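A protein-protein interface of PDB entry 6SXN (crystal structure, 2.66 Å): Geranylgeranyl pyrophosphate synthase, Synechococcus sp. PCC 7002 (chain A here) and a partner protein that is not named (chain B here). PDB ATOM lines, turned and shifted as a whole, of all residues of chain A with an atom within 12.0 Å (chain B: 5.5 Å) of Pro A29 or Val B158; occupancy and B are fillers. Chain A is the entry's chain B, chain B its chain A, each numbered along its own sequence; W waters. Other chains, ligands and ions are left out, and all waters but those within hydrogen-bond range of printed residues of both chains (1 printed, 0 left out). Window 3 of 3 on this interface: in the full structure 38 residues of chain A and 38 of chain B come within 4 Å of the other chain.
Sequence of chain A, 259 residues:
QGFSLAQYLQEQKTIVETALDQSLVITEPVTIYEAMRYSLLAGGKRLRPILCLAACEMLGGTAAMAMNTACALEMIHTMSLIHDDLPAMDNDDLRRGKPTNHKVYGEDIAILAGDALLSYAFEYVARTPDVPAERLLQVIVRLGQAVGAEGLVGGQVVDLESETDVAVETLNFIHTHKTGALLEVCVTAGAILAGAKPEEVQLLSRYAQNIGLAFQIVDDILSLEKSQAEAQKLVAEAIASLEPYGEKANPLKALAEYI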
ATOM      1  N   LEU A  24     -19.704 -30.051 -19.434  1.00  0.00           N
ATOM      2  CA  LEU A  24     -18.491 -29.456 -19.972  1.00  0.00           C
ATOM      3  C   LEU A  24     -17.368 -30.484 -19.927  1.00  0.00           C
ATOM      4  O   LEU A  24     -16.584 -30.503 -18.987  1.00  0.00           O
ATOM      5  CB  LEU A  24     -18.147 -28.229 -19.128  1.00  0.00           C
ATOM      6  CG  LEU A  24     -18.472 -26.850 -19.689  1.00  0.00           C
ATOM      7  CD1 LEU A  24     -19.527 -26.886 -20.756  1.00  0.00           C
ATOM      8  CD2 LEU A  24     -18.907 -25.903 -18.582  1.00  0.00           C
ATOM      9  N   VAL A  25     -17.272 -31.326 -20.964  1.00  0.00           N
ATOM     10  CA  VAL A  25     -16.168 -32.274 -21.092  1.00  0.00           C
ATOM     11  C   VAL A  25     -15.003 -31.606 -21.828  1.00  0.00           C
ATOM     12  O   VAL A  25     -15.165 -31.043 -22.907  1.00  0.00           O
ATOM     13  CB  VAL A  25     -16.625 -33.604 -21.736  1.00  0.00           C
ATOM     14  CG1 VAL A  25     -17.616 -33.405 -22.882  1.00  0.00           C
ATOM     15  CG2 VAL A  25     -15.443 -34.445 -22.201  1.00  0.00           C
ATOM     16  N   ILE A  26     -13.820 -31.698 -21.222  1.00  0.00           N
ATOM     17  CA  ILE A  26     -12.630 -30.936 -21.592  1.00  0.00           C
ATOM     18  C   ILE A  26     -11.967 -31.547 -22.832  1.00  0.00           C
ATOM     19  O   ILE A  26     -11.381 -32.596 -22.740  1.00  0.00           O
ATOM     20  CB  ILE A  26     -11.660 -30.855 -20.389  1.00  0.00           C
ATOM     21  CG1 ILE A  26     -12.345 -30.573 -19.046  1.00  0.00           C
ATOM     22  CG2 ILE A  26     -10.561 -29.858 -20.657  1.00  0.00           C
ATOM     23  CD1 ILE A  26     -12.973 -31.842 -18.402  1.00  0.00           C
ATOM     24  N   THR A  27     -11.826 -30.738 -23.883  1.00  0.00           N
ATOM     25  CA  THR A  27     -11.170 -31.164 -25.142  1.00  0.00           C
ATOM     26  C   THR A  27     -10.390 -30.011 -25.776  1.00  0.00           C
ATOM     27  O   THR A  27     -10.110 -29.032 -25.104  1.00  0.00           O
ATOM     28  CB  THR A  27     -12.221 -31.599 -26.169  1.00  0.00           C
ATOM     29  N   GLU A  28     -10.057 -30.202 -27.049  1.00  0.00           N
ATOM     30  CA  GLU A  28      -9.408 -29.276 -28.020  1.00  0.00           C
ATOM     31  C   GLU A  28      -8.507 -28.230 -27.367  1.00  0.00           C
ATOM     32  O   GLU A  28      -7.366 -28.580 -27.035  1.00  0.00           O
ATOM     33  CB  GLU A  28     -10.486 -28.605 -28.872  1.00  0.00           C
ATOM     34  CG  GLU A  28     -10.477 -29.034 -30.340  1.00  0.00           C
ATOM     35  CD  GLU A  28     -10.595 -30.505 -30.732  1.00  0.00           C
ATOM     36  OE1 GLU A  28     -10.109 -30.858 -31.822  1.00  0.00           O
ATOM     37  OE2 GLU A  28     -11.188 -31.289 -29.977  1.00  0.00           O
ATOM     38  N   PRO A  29      -8.919 -26.946 -27.298  1.00  0.00           N
ATOM     39  CA  PRO A  29      -8.267 -25.965 -26.435  1.00  0.00           C
ATOM     40  C   PRO A  29      -8.763 -26.111 -24.996  1.00  0.00           C
ATOM     41  O   PRO A  29      -9.781 -25.609 -24.698  1.00  0.00           O
ATOM     42  CB  PRO A  29      -8.732 -24.627 -27.002  1.00  0.00           C
ATOM     43  CG  PRO A  29     -10.060 -24.932 -27.622  1.00  0.00           C
ATOM     44  CD  PRO A  29      -9.985 -26.367 -28.093  1.00  0.00           C
ATOM     45  N   VAL A  30      -7.993 -26.783 -24.151  1.00  0.00           N
ATOM     46  CA  VAL A  30      -8.406 -27.036 -22.746  1.00  0.00           C
ATOM     47  C   VAL A  30      -8.590 -25.744 -21.952  1.00  0.00           C
ATOM     48  O   VAL A  30      -9.374 -25.776 -21.029  1.00  0.00           O
ATOM     49  CB  VAL A  30      -7.442 -28.001 -22.040  1.00  0.00           C
ATOM     50  CG1 VAL A  30      -7.118 -29.191 -22.910  1.00  0.00           C
ATOM     51  CG2 VAL A  30      -6.180 -27.312 -21.574  1.00  0.00           C
ATOM     52  N   THR A  31      -7.906 -24.656 -22.298  1.00  0.00           N
ATOM     53  CA  THR A  31      -8.023 -23.431 -21.522  1.00  0.00           C
ATOM     54  C   THR A  31      -9.466 -22.886 -21.538  1.00  0.00           C
ATOM     55  O   THR A  31      -9.952 -22.431 -20.512  1.00  0.00           O
ATOM     56  CB  THR A  31      -6.787 -22.518 -21.689  1.00  0.00           C
ATOM     57  OG1 THR A  31      -7.273 -21.186 -21.879  1.00  0.00           O
ATOM     58  CG2 THR A  31      -5.860 -22.933 -22.818  1.00  0.00           C
ATOM     59  N   ILE A  32     -10.186 -22.972 -22.663  1.00  0.00           N
ATOM     60  CA  ILE A  32     -11.527 -22.423 -22.707  1.00  0.00           C
ATOM     61  C   ILE A  32     -12.449 -23.224 -21.794  1.00  0.00           C
ATOM     62  O   ILE A  32     -13.204 -22.640 -21.007  1.00  0.00           O
ATOM     63  CB  ILE A  32     -12.076 -22.270 -24.137  1.00  0.00           C
ATOM     64  CG1 ILE A  32     -13.305 -21.367 -24.164  1.00  0.00           C
ATOM     65  CG2 ILE A  32     -12.405 -23.618 -24.752  1.00  0.00           C
ATOM     66  CD1 ILE A  32     -13.026 -19.961 -23.677  1.00  0.00           C
ATOM     67  N   TYR A  33     -12.374 -24.560 -21.883  1.00  0.00           N
ATOM     68  CA  TYR A  33     -13.197 -25.405 -21.029  1.00  0.00           C
ATOM     69  C   TYR A  33     -12.837 -25.193 -19.552  1.00  0.00           C
ATOM     70  O   TYR A  33     -13.702 -25.226 -18.684  1.00  0.00           O
ATOM     71  CB  TYR A  33     -13.048 -26.859 -21.453  1.00  0.00           C
ATOM     72  CG  TYR A  33     -13.631 -27.145 -22.806  1.00  0.00           C
ATOM     73  CD1 TYR A  33     -14.994 -27.386 -22.953  1.00  0.00           C
ATOM     74  CD2 TYR A  33     -12.832 -27.173 -23.937  1.00  0.00           C
ATOM     75  CE1 TYR A  33     -15.549 -27.639 -24.188  1.00  0.00           C
ATOM     76  CE2 TYR A  33     -13.381 -27.442 -25.183  1.00  0.00           C
ATOM     77  CZ  TYR A  33     -14.746 -27.660 -25.310  1.00  0.00           C
ATOM     78  OH  TYR A  33     -15.282 -27.870 -26.559  1.00  0.00           O
ATOM     79  N   GLU A  34     -11.546 -24.986 -19.273  1.00  0.00           N
ATOM     80  CA  GLU A  34     -11.075 -24.756 -17.924  1.00  0.00           C
ATOM     81  C   GLU A  34     -11.712 -23.490 -17.387  1.00  0.00           C
ATOM     82  O   GLU A  34     -12.268 -23.480 -16.289  1.00  0.00           O
ATOM     83  CB  GLU A  34      -9.557 -24.632 -17.906  1.00  0.00           C
ATOM     84  CG  GLU A  34      -8.874 -25.974 -17.634  1.00  0.00           C
ATOM     85  CD  GLU A  34      -7.373 -25.875 -17.802  1.00  0.00           C
ATOM     86  OE1 GLU A  34      -6.777 -24.927 -17.258  1.00  0.00           O
ATOM     87  OE2 GLU A  34      -6.826 -26.707 -18.513  1.00  0.00           O
ATOM     88  N   ALA A  35     -11.654 -22.429 -18.192  1.00  0.00           N
ATOM     89  CA  ALA A  35     -12.176 -21.120 -17.807  1.00  0.00           C
ATOM     90  C   ALA A  35     -13.689 -21.177 -17.593  1.00  0.00           C
ATOM     91  O   ALA A  35     -14.215 -20.535 -16.696  1.00  0.00           O
ATOM     92  CB  ALA A  35     -11.783 -20.086 -18.836  1.00  0.00           C
ATOM     93  N   MET A  36     -14.381 -21.967 -18.406  1.00  0.00           N
ATOM     94  CA  MET A  36     -15.821 -22.134 -18.276  1.00  0.00           C
ATOM     95  C   MET A  36     -16.138 -22.886 -16.989  1.00  0.00           C
ATOM     96  O   MET A  36     -16.974 -22.448 -16.201  1.00  0.00           O
ATOM     97  CB  MET A  36     -16.413 -22.899 -19.469  1.00  0.00           C
ATOM     98  CG  MET A  36     -16.286 -22.174 -20.810  1.00  0.00           C
ATOM     99  SD  MET A  36     -17.171 -22.999 -22.123  1.00  0.00           S
ATOM    100  CE  MET A  36     -15.898 -24.074 -22.752  1.00  0.00           C
ATOM    101  N   ARG A  37     -15.447 -24.011 -16.781  1.00  0.00           N
ATOM    102  CA  ARG A  37     -15.715 -24.880 -15.649  1.00  0.00           C
ATOM    103  C   ARG A  37     -15.415 -24.140 -14.348  1.00  0.00           C
ATOM    104  O   ARG A  37     -16.105 -24.330 -13.334  1.00  0.00           O
ATOM    105  CB  ARG A  37     -14.934 -26.182 -15.794  1.00  0.00           C
ATOM    106  CG  ARG A  37     -15.480 -27.086 -16.895  1.00  0.00           C
ATOM    107  CD  ARG A  37     -14.529 -28.283 -17.173  1.00  0.00           C
ATOM    108  NE  ARG A  37     -14.362 -29.054 -15.959  1.00  0.00           N
ATOM    109  CZ  ARG A  37     -15.208 -29.976 -15.533  1.00  0.00           C
ATOM    110  NH1 ARG A  37     -16.261 -30.293 -16.252  1.00  0.00           N
ATOM    111  NH2 ARG A  37     -14.995 -30.590 -14.379  1.00  0.00           N
ATOM    112  N   TYR A  38     -14.395 -23.281 -14.402  1.00  0.00           N
ATOM    113  CA  TYR A  38     -13.962 -22.543 -13.224  1.00  0.00           C
ATOM    114  C   TYR A  38     -15.118 -21.744 -12.648  1.00  0.00           C
ATOM    115  O   TYR A  38     -15.377 -21.797 -11.452  1.00  0.00           O
ATOM    116  CB  TYR A  38     -12.817 -21.585 -13.546  1.00  0.00           C
ATOM    117  CG  TYR A  38     -12.355 -20.761 -12.368  1.00  0.00           C
ATOM    118  CD1 TYR A  38     -11.662 -21.322 -11.304  1.00  0.00           C
ATOM    119  CD2 TYR A  38     -12.615 -19.396 -12.329  1.00  0.00           C
ATOM    120  CE1 TYR A  38     -11.231 -20.554 -10.233  1.00  0.00           C
ATOM    121  CE2 TYR A  38     -12.130 -18.598 -11.297  1.00  0.00           C
ATOM    122  CZ  TYR A  38     -11.441 -19.179 -10.240  1.00  0.00           C
ATOM    123  OH  TYR A  38     -11.020 -18.382  -9.206  1.00  0.00           O
ATOM    124  N   TYR A 105      -7.602 -16.047 -15.892  1.00  0.00           N
ATOM    125  CA  TYR A 105      -7.368 -16.496 -17.266  1.00  0.00           C
ATOM    126  C   TYR A 105      -7.088 -15.345 -18.224  1.00  0.00           C
ATOM    127  O   TYR A 105      -6.671 -15.589 -19.355  1.00  0.00           O
ATOM    128  CB  TYR A 105      -8.533 -17.341 -17.801  1.00  0.00           C
ATOM    129  CG  TYR A 105      -8.746 -18.620 -17.038  1.00  0.00           C
ATOM    130  CD1 TYR A 105      -8.064 -19.779 -17.384  1.00  0.00           C
ATOM    131  CD2 TYR A 105      -9.618 -18.668 -15.962  1.00  0.00           C
ATOM    132  CE1 TYR A 105      -8.250 -20.966 -16.691  1.00  0.00           C
ATOM    133  CE2 TYR A 105      -9.819 -19.840 -15.258  1.00  0.00           C
ATOM    134  CZ  TYR A 105      -9.134 -20.988 -15.628  1.00  0.00           C
ATOM    135  OH  TYR A 105      -9.339 -22.149 -14.949  1.00  0.00           O
ATOM    136  N   ASP A 108      -9.463 -11.463 -22.001  1.00  0.00           N
ATOM    137  CA  ASP A 108      -9.784 -12.015 -23.308  1.00  0.00           C
ATOM    138  C   ASP A 108     -10.478 -13.366 -23.165  1.00  0.00           C
ATOM    139  O   ASP A 108     -11.561 -13.557 -23.708  1.00  0.00           O
ATOM    140  CB  ASP A 108      -8.577 -12.021 -24.260  1.00  0.00           C
ATOM    141  CG  ASP A 108      -7.310 -12.712 -23.759  1.00  0.00           C
ATOM    142  OD1 ASP A 108      -7.274 -13.185 -22.559  1.00  0.00           O
ATOM    143  OD2 ASP A 108      -6.381 -12.837 -24.603  1.00  0.00           O
ATOM    144  N   ILE A 109      -9.854 -14.274 -22.412  1.00  0.00           N
ATOM    145  CA  ILE A 109     -10.378 -15.619 -22.228  1.00  0.00           C
ATOM    146  C   ILE A 109     -11.725 -15.515 -21.513  1.00  0.00           C
ATOM    147  O   ILE A 109     -12.658 -16.233 -21.849  1.00  0.00           O
ATOM    148  CB  ILE A 109      -9.364 -16.519 -21.484  1.00  0.00           C
ATOM    149  CG1 ILE A 109      -8.086 -16.732 -22.312  1.00  0.00           C
ATOM    150  CG2 ILE A 109      -9.999 -17.839 -21.052  1.00  0.00           C
ATOM    151  CD1 ILE A 109      -8.242 -17.588 -23.549  1.00  0.00           C
ATOM    152  N   ALA A 110     -11.828 -14.604 -20.537  1.00  0.00           N
ATOM    153  CA  ALA A 110     -13.056 -14.437 -19.769  1.00  0.00           C
ATOM    154  C   ALA A 110     -14.203 -14.071 -20.703  1.00  0.00           C
ATOM    155  O   ALA A 110     -15.266 -14.669 -20.616  1.00  0.00           O
ATOM    156  CB  ALA A 110     -12.873 -13.426 -18.678  1.00  0.00           C
ATOM    157  N   LEU A 112     -14.463 -14.626 -23.895  1.00  0.00           N
ATOM    158  CA  LEU A 112     -14.762 -15.796 -24.715  1.00  0.00           C
ATOM    159  C   LEU A 112     -15.448 -16.899 -23.896  1.00  0.00           C
ATOM    160  O   LEU A 112     -16.327 -17.585 -24.390  1.00  0.00           O
ATOM    161  CB  LEU A 112     -13.460 -16.265 -25.379  1.00  0.00           C
ATOM    162  CG  LEU A 112     -12.838 -15.251 -26.341  1.00  0.00           C
ATOM    163  CD1 LEU A 112     -11.491 -15.716 -26.848  1.00  0.00           C
ATOM    164  CD2 LEU A 112     -13.773 -15.046 -27.529  1.00  0.00           C
ATOM    165  N   ALA A 113     -15.079 -17.048 -22.622  1.00  0.00           N
ATOM    166  CA  ALA A 113     -15.668 -18.091 -21.809  1.00  0.00           C
ATOM    167  C   ALA A 113     -17.164 -17.811 -21.631  1.00  0.00           C
ATOM    168  O   ALA A 113     -18.016 -18.718 -21.680  1.00  0.00           O
ATOM    169  CB  ALA A 113     -14.946 -18.197 -20.490  1.00  0.00           C
ATOM    170  N   ALA A 116     -18.955 -18.539 -24.946  1.00  0.00           N
ATOM    171  CA  ALA A 116     -19.085 -19.979 -25.105  1.00  0.00           C
ATOM    172  C   ALA A 116     -20.261 -20.511 -24.270  1.00  0.00           C
ATOM    173  O   ALA A 116     -21.073 -21.294 -24.787  1.00  0.00           O
ATOM    174  CB  ALA A 116     -17.788 -20.656 -24.723  1.00  0.00           C
ATOM    175  N   ALA B 149     -17.121 -23.317 -28.087  1.00  0.00           N
ATOM    176  CA  ALA B 149     -15.796 -23.857 -27.820  1.00  0.00           C
ATOM    177  C   ALA B 149     -15.340 -24.811 -28.928  1.00  0.00           C
ATOM    178  O   ALA B 149     -14.146 -24.924 -29.197  1.00  0.00           O
ATOM    179  CB  ALA B 149     -15.812 -24.555 -26.505  1.00  0.00           C
ATOM    180  N   VAL B 153     -15.380 -19.651 -31.048  1.00  0.00           N
ATOM    181  CA  VAL B 153     -14.704 -19.217 -29.839  1.00  0.00           C
ATOM    182  C   VAL B 153     -13.467 -20.089 -29.627  1.00  0.00           C
ATOM    183  O   VAL B 153     -12.412 -19.590 -29.246  1.00  0.00           O
ATOM    184  CB  VAL B 153     -15.646 -19.279 -28.623  1.00  0.00           C
ATOM    185  CG1 VAL B 153     -14.893 -19.126 -27.305  1.00  0.00           C
ATOM    186  CG2 VAL B 153     -16.754 -18.258 -28.705  1.00  0.00           C
ATOM    187  N   GLY B 154     -13.610 -21.404 -29.864  1.00  0.00           N
ATOM    188  CA  GLY B 154     -12.482 -22.318 -29.813  1.00  0.00           C
ATOM    189  C   GLY B 154     -11.315 -21.826 -30.648  1.00  0.00           C
ATOM    190  O   GLY B 154     -10.196 -21.761 -30.149  1.00  0.00           O
ATOM    191  N   GLY B 155     -11.589 -21.496 -31.919  1.00  0.00           N
ATOM    192  CA  GLY B 155     -10.592 -20.930 -32.819  1.00  0.00           C
ATOM    193  C   GLY B 155      -9.929 -19.683 -32.246  1.00  0.00           C
ATOM    194  O   GLY B 155      -8.717 -19.614 -32.173  1.00  0.00           O
ATOM    195  N   GLN B 156     -10.743 -18.714 -31.816  1.00  0.00           N
ATOM    196  CA  GLN B 156     -10.228 -17.470 -31.285  1.00  0.00           C
ATOM    197  C   GLN B 156      -9.295 -17.765 -30.099  1.00  0.00           C
ATOM    198  O   GLN B 156      -8.294 -17.077 -29.924  1.00  0.00           O
ATOM    199  CB  GLN B 156     -11.393 -16.484 -31.087  1.00  0.00           C
ATOM    200  CG  GLN B 156     -11.000 -15.081 -30.621  1.00  0.00           C
ATOM    201  CD  GLN B 156      -9.936 -14.381 -31.437  1.00  0.00           C
ATOM    202  OE1 GLN B 156      -9.811 -14.557 -32.646  1.00  0.00           O
ATOM    203  NE2 GLN B 156      -9.156 -13.533 -30.787  1.00  0.00           N
ATOM    204  N   VAL B 157      -9.581 -18.808 -29.308  1.00  0.00           N
ATOM    205  CA  VAL B 157      -8.777 -19.088 -28.124  1.00  0.00           C
ATOM    206  C   VAL B 157      -7.394 -19.595 -28.534  1.00  0.00           C
ATOM    207  O   VAL B 157      -6.390 -19.110 -28.006  1.00  0.00           O
ATOM    208  CB  VAL B 157      -9.455 -20.046 -27.123  1.00  0.00           C
ATOM    209  CG1 VAL B 157      -8.446 -20.628 -26.141  1.00  0.00           C
ATOM    210  CG2 VAL B 157     -10.580 -19.361 -26.360  1.00  0.00           C
ATOM    211  N   VAL B 158      -7.358 -20.564 -29.469  1.00  0.00           N
ATOM    212  CA  VAL B 158      -6.123 -21.122 -29.994  1.00  0.00           C
ATOM    213  C   VAL B 158      -5.309 -20.018 -30.674  1.00  0.00           C
ATOM    214  O   VAL B 158      -4.094 -19.971 -30.526  1.00  0.00           O
ATOM    215  CB  VAL B 158      -6.401 -22.290 -30.950  1.00  0.00           C
ATOM    216  CG1 VAL B 158      -5.149 -22.781 -31.657  1.00  0.00           C
ATOM    217  CG2 VAL B 158      -7.101 -23.436 -30.227  1.00  0.00           C
ATOM    218  N   ASP B 159      -5.998 -19.140 -31.414  1.00  0.00           N
ATOM    219  CA  ASP B 159      -5.416 -18.000 -32.092  1.00  0.00           C
ATOM    220  C   ASP B 159      -4.679 -17.142 -31.066  1.00  0.00           C
ATOM    221  O   ASP B 159      -3.545 -16.737 -31.292  1.00  0.00           O
ATOM    222  CB  ASP B 159      -6.491 -17.203 -32.833  1.00  0.00           C
ATOM    223  CG  ASP B 159      -6.003 -16.169 -33.843  1.00  0.00           C
ATOM    224  OD1 ASP B 159      -4.797 -15.859 -33.878  1.00  0.00           O
ATOM    225  OD2 ASP B 159      -6.849 -15.627 -34.544  1.00  0.00           O
ATOM    226  N   LEU B 160      -5.323 -16.862 -29.933  1.00  0.00           N
ATOM    227  CA  LEU B 160      -4.754 -15.947 -28.954  1.00  0.00           C
ATOM    228  C   LEU B 160      -3.518 -16.578 -28.319  1.00  0.00           C
ATOM    229  O   LEU B 160      -2.544 -15.892 -28.049  1.00  0.00           O
ATOM    230  CB  LEU B 160      -5.805 -15.571 -27.906  1.00  0.00           C
ATOM    231  CG  LEU B 160      -6.802 -14.509 -28.344  1.00  0.00           C
ATOM    232  CD1 LEU B 160      -7.890 -14.350 -27.288  1.00  0.00           C
ATOM    233  CD2 LEU B 160      -6.123 -13.181 -28.651  1.00  0.00           C
ATOM    234  N   GLU B 161      -3.579 -17.890 -28.108  1.00  0.00           N
ATOM    235  CA  GLU B 161      -2.525 -18.639 -27.452  1.00  0.00           C
ATOM    236  C   GLU B 161      -1.295 -18.759 -28.356  1.00  0.00           C
ATOM    237  O   GLU B 161      -0.182 -18.964 -27.892  1.00  0.00           O
ATOM    238  CB  GLU B 161      -3.050 -19.988 -26.963  1.00  0.00           C
ATOM    239  CG  GLU B 161      -2.248 -20.521 -25.780  1.00  0.00           C
ATOM    240  CD  GLU B 161      -0.842 -21.024 -26.064  1.00  0.00           C
ATOM    241  OE1 GLU B 161      -0.682 -21.659 -27.120  1.00  0.00           O
ATOM    242  OE2 GLU B 161       0.087 -20.714 -25.272  1.00  0.00           O
ATOM    243  N   SER B 162      -1.482 -18.536 -29.663  1.00  0.00           N
ATOM    244  CA  SER B 162      -0.401 -18.642 -30.630  1.00  0.00           C
ATOM    245  C   SER B 162       0.053 -17.264 -31.099  1.00  0.00           C
ATOM    246  O   SER B 162       0.981 -17.172 -31.902  1.00  0.00           O
ATOM    247  CB  SER B 162      -0.815 -19.489 -31.794  1.00  0.00           C
ATOM    248  OG  SER B 162      -1.178 -20.792 -31.353  1.00  0.00           O
ATOM    249  N   GLU B 163      -0.606 -16.185 -30.641  1.00  0.00           N
ATOM    250  CA  GLU B 163      -0.076 -14.842 -30.837  1.00  0.00           C
ATOM    251  C   GLU B 163       1.328 -14.751 -30.240  1.00  0.00           C
ATOM    252  O   GLU B 163       2.103 -13.899 -30.655  1.00  0.00           O
ATOM    253  CB  GLU B 163      -1.006 -13.711 -30.383  1.00  0.00           C
ATOM    254  N   LEU B 172      -1.614 -25.672 -36.430  1.00  0.00           N
ATOM    255  CA  LEU B 172      -2.121 -24.647 -35.531  1.00  0.00           C
ATOM    256  C   LEU B 172      -2.780 -23.542 -36.353  1.00  0.00           C
ATOM    257  O   LEU B 172      -3.655 -22.825 -35.866  1.00  0.00           O
ATOM    258  CB  LEU B 172      -0.999 -24.088 -34.646  1.00  0.00           C
ATOM    259  CG  LEU B 172      -0.749 -24.785 -33.305  1.00  0.00           C
ATOM    260  CD1 LEU B 172      -2.024 -25.006 -32.500  1.00  0.00           C
ATOM    261  CD2 LEU B 172      -0.012 -26.103 -33.480  1.00  0.00           C
ATOM    262  N   ILE B 175      -6.348 -25.188 -37.342  1.00  0.00           N
ATOM    263  CA  ILE B 175      -7.422 -25.151 -36.316  1.00  0.00           C
ATOM    264  C   ILE B 175      -7.988 -23.725 -36.252  1.00  0.00           C
ATOM    265  O   ILE B 175      -9.214 -23.583 -36.177  1.00  0.00           O
ATOM    266  CB  ILE B 175      -6.879 -25.704 -34.988  1.00  0.00           C
ATOM    267  CG1 ILE B 175      -7.874 -25.578 -33.836  1.00  0.00           C
ATOM    268  CG2 ILE B 175      -5.528 -25.093 -34.671  1.00  0.00           C
ATOM    269  CD1 ILE B 175      -8.225 -26.897 -33.202  1.00  0.00           C
ATOM    270  N   HIS B 176      -7.153 -22.693 -36.356  1.00  0.00           N
ATOM    271  CA  HIS B 176      -7.713 -21.316 -36.314  1.00  0.00           C
ATOM    272  C   HIS B 176      -8.671 -21.114 -37.493  1.00  0.00           C
ATOM    273  O   HIS B 176      -9.819 -20.679 -37.274  1.00  0.00           O
ATOM    274  CB  HIS B 176      -6.593 -20.275 -36.263  1.00  0.00           C
HETATM  275  O   HOH W   1     -19.768 -23.821 -26.441  1.00  0.00           O
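OG of Ser B162 is in hydrogen-bond range of O of Val B158, at 3.1 Å.
CG2 of Val B158 touches CB of Pro A29 (3.8 Å).
Ala B149 touches Ile A32 (CB to CG2, 3.9 Å).
Ile A32 touches Val B157.
Tyr A33 touches Ala B149 (OH to CB, 3.4 Å).
Met A36 touches Ala B149 (CE to CB, 3.8 Å).
Leu B160 touches Asp A108 (CD1 to OD2, 3.4 Å).
Val B153 touches Leu A112.
Gln B156 touches Leu A112 (CG to CD1, 3.9 Å).
Leu A112 touches Val B157.
Leu A112 touches Leu B160 (CD1 to CD1, 3.9 Å).
Val A25 touches none of the printed residues of chain B.
Of chain B, only Val B158 (3.8 Å) comes within 4 Å of Pro A29.
Of the printed residues of chain B, Ile A32 touches Ala B149 and Val B157.
Of the printed residues of chain B, Tyr A33 touches Ala B149 (3.4 Å).
Of the printed residues of chain B, Met A36 touches Ala B149 (3.8 Å).
Ala B149 touches three residues of chain A.
Printed residues of chain A within 4 Å of Val B153: Leu A112 (3.6 Å).
Gln B156 touches one residue of chain A.
Of chain A, only Pro A29 comes within 4 Å of Val B158.
Asp B159 touches none of the printed residues of chain A.
Leu B160 touches just these residues of chain A: Asp A108 (3.4 Å) and Leu A112 (3.9 Å).
Glu B161 touches none of the printed residues of chain A.
No residue of chain A comes within 4 Å of Ser B162.
No residue of chain A comes within 4 Å of Ile B175.
No residue of chain A comes within 4 Å of His B176.
The nearest residue of chain A that does not touch Val B158 is Glu A28 (5.8 Å).
Of the 22 printed residues of chain A, 6 touch a printed residue of chain B.
Hydrophobic or aromatic side chains of chain A within 4 Å of the printed part of chain B: Pro A29, Ile A32, Tyr A33, Met A36 and Leu A112.
Among the printed residues, 10 pairs touch across the chains.
Among the printed residues, no Asp or Glu carboxylate lies within 4 Å of a Lys or Arg side-chain nitrogen of the other chain.
Water W1 bridges the backbone NH of Ala B149 (3.2 Å) and the backbone carbonyl oxygen of Ala A116 (3.3 Å).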
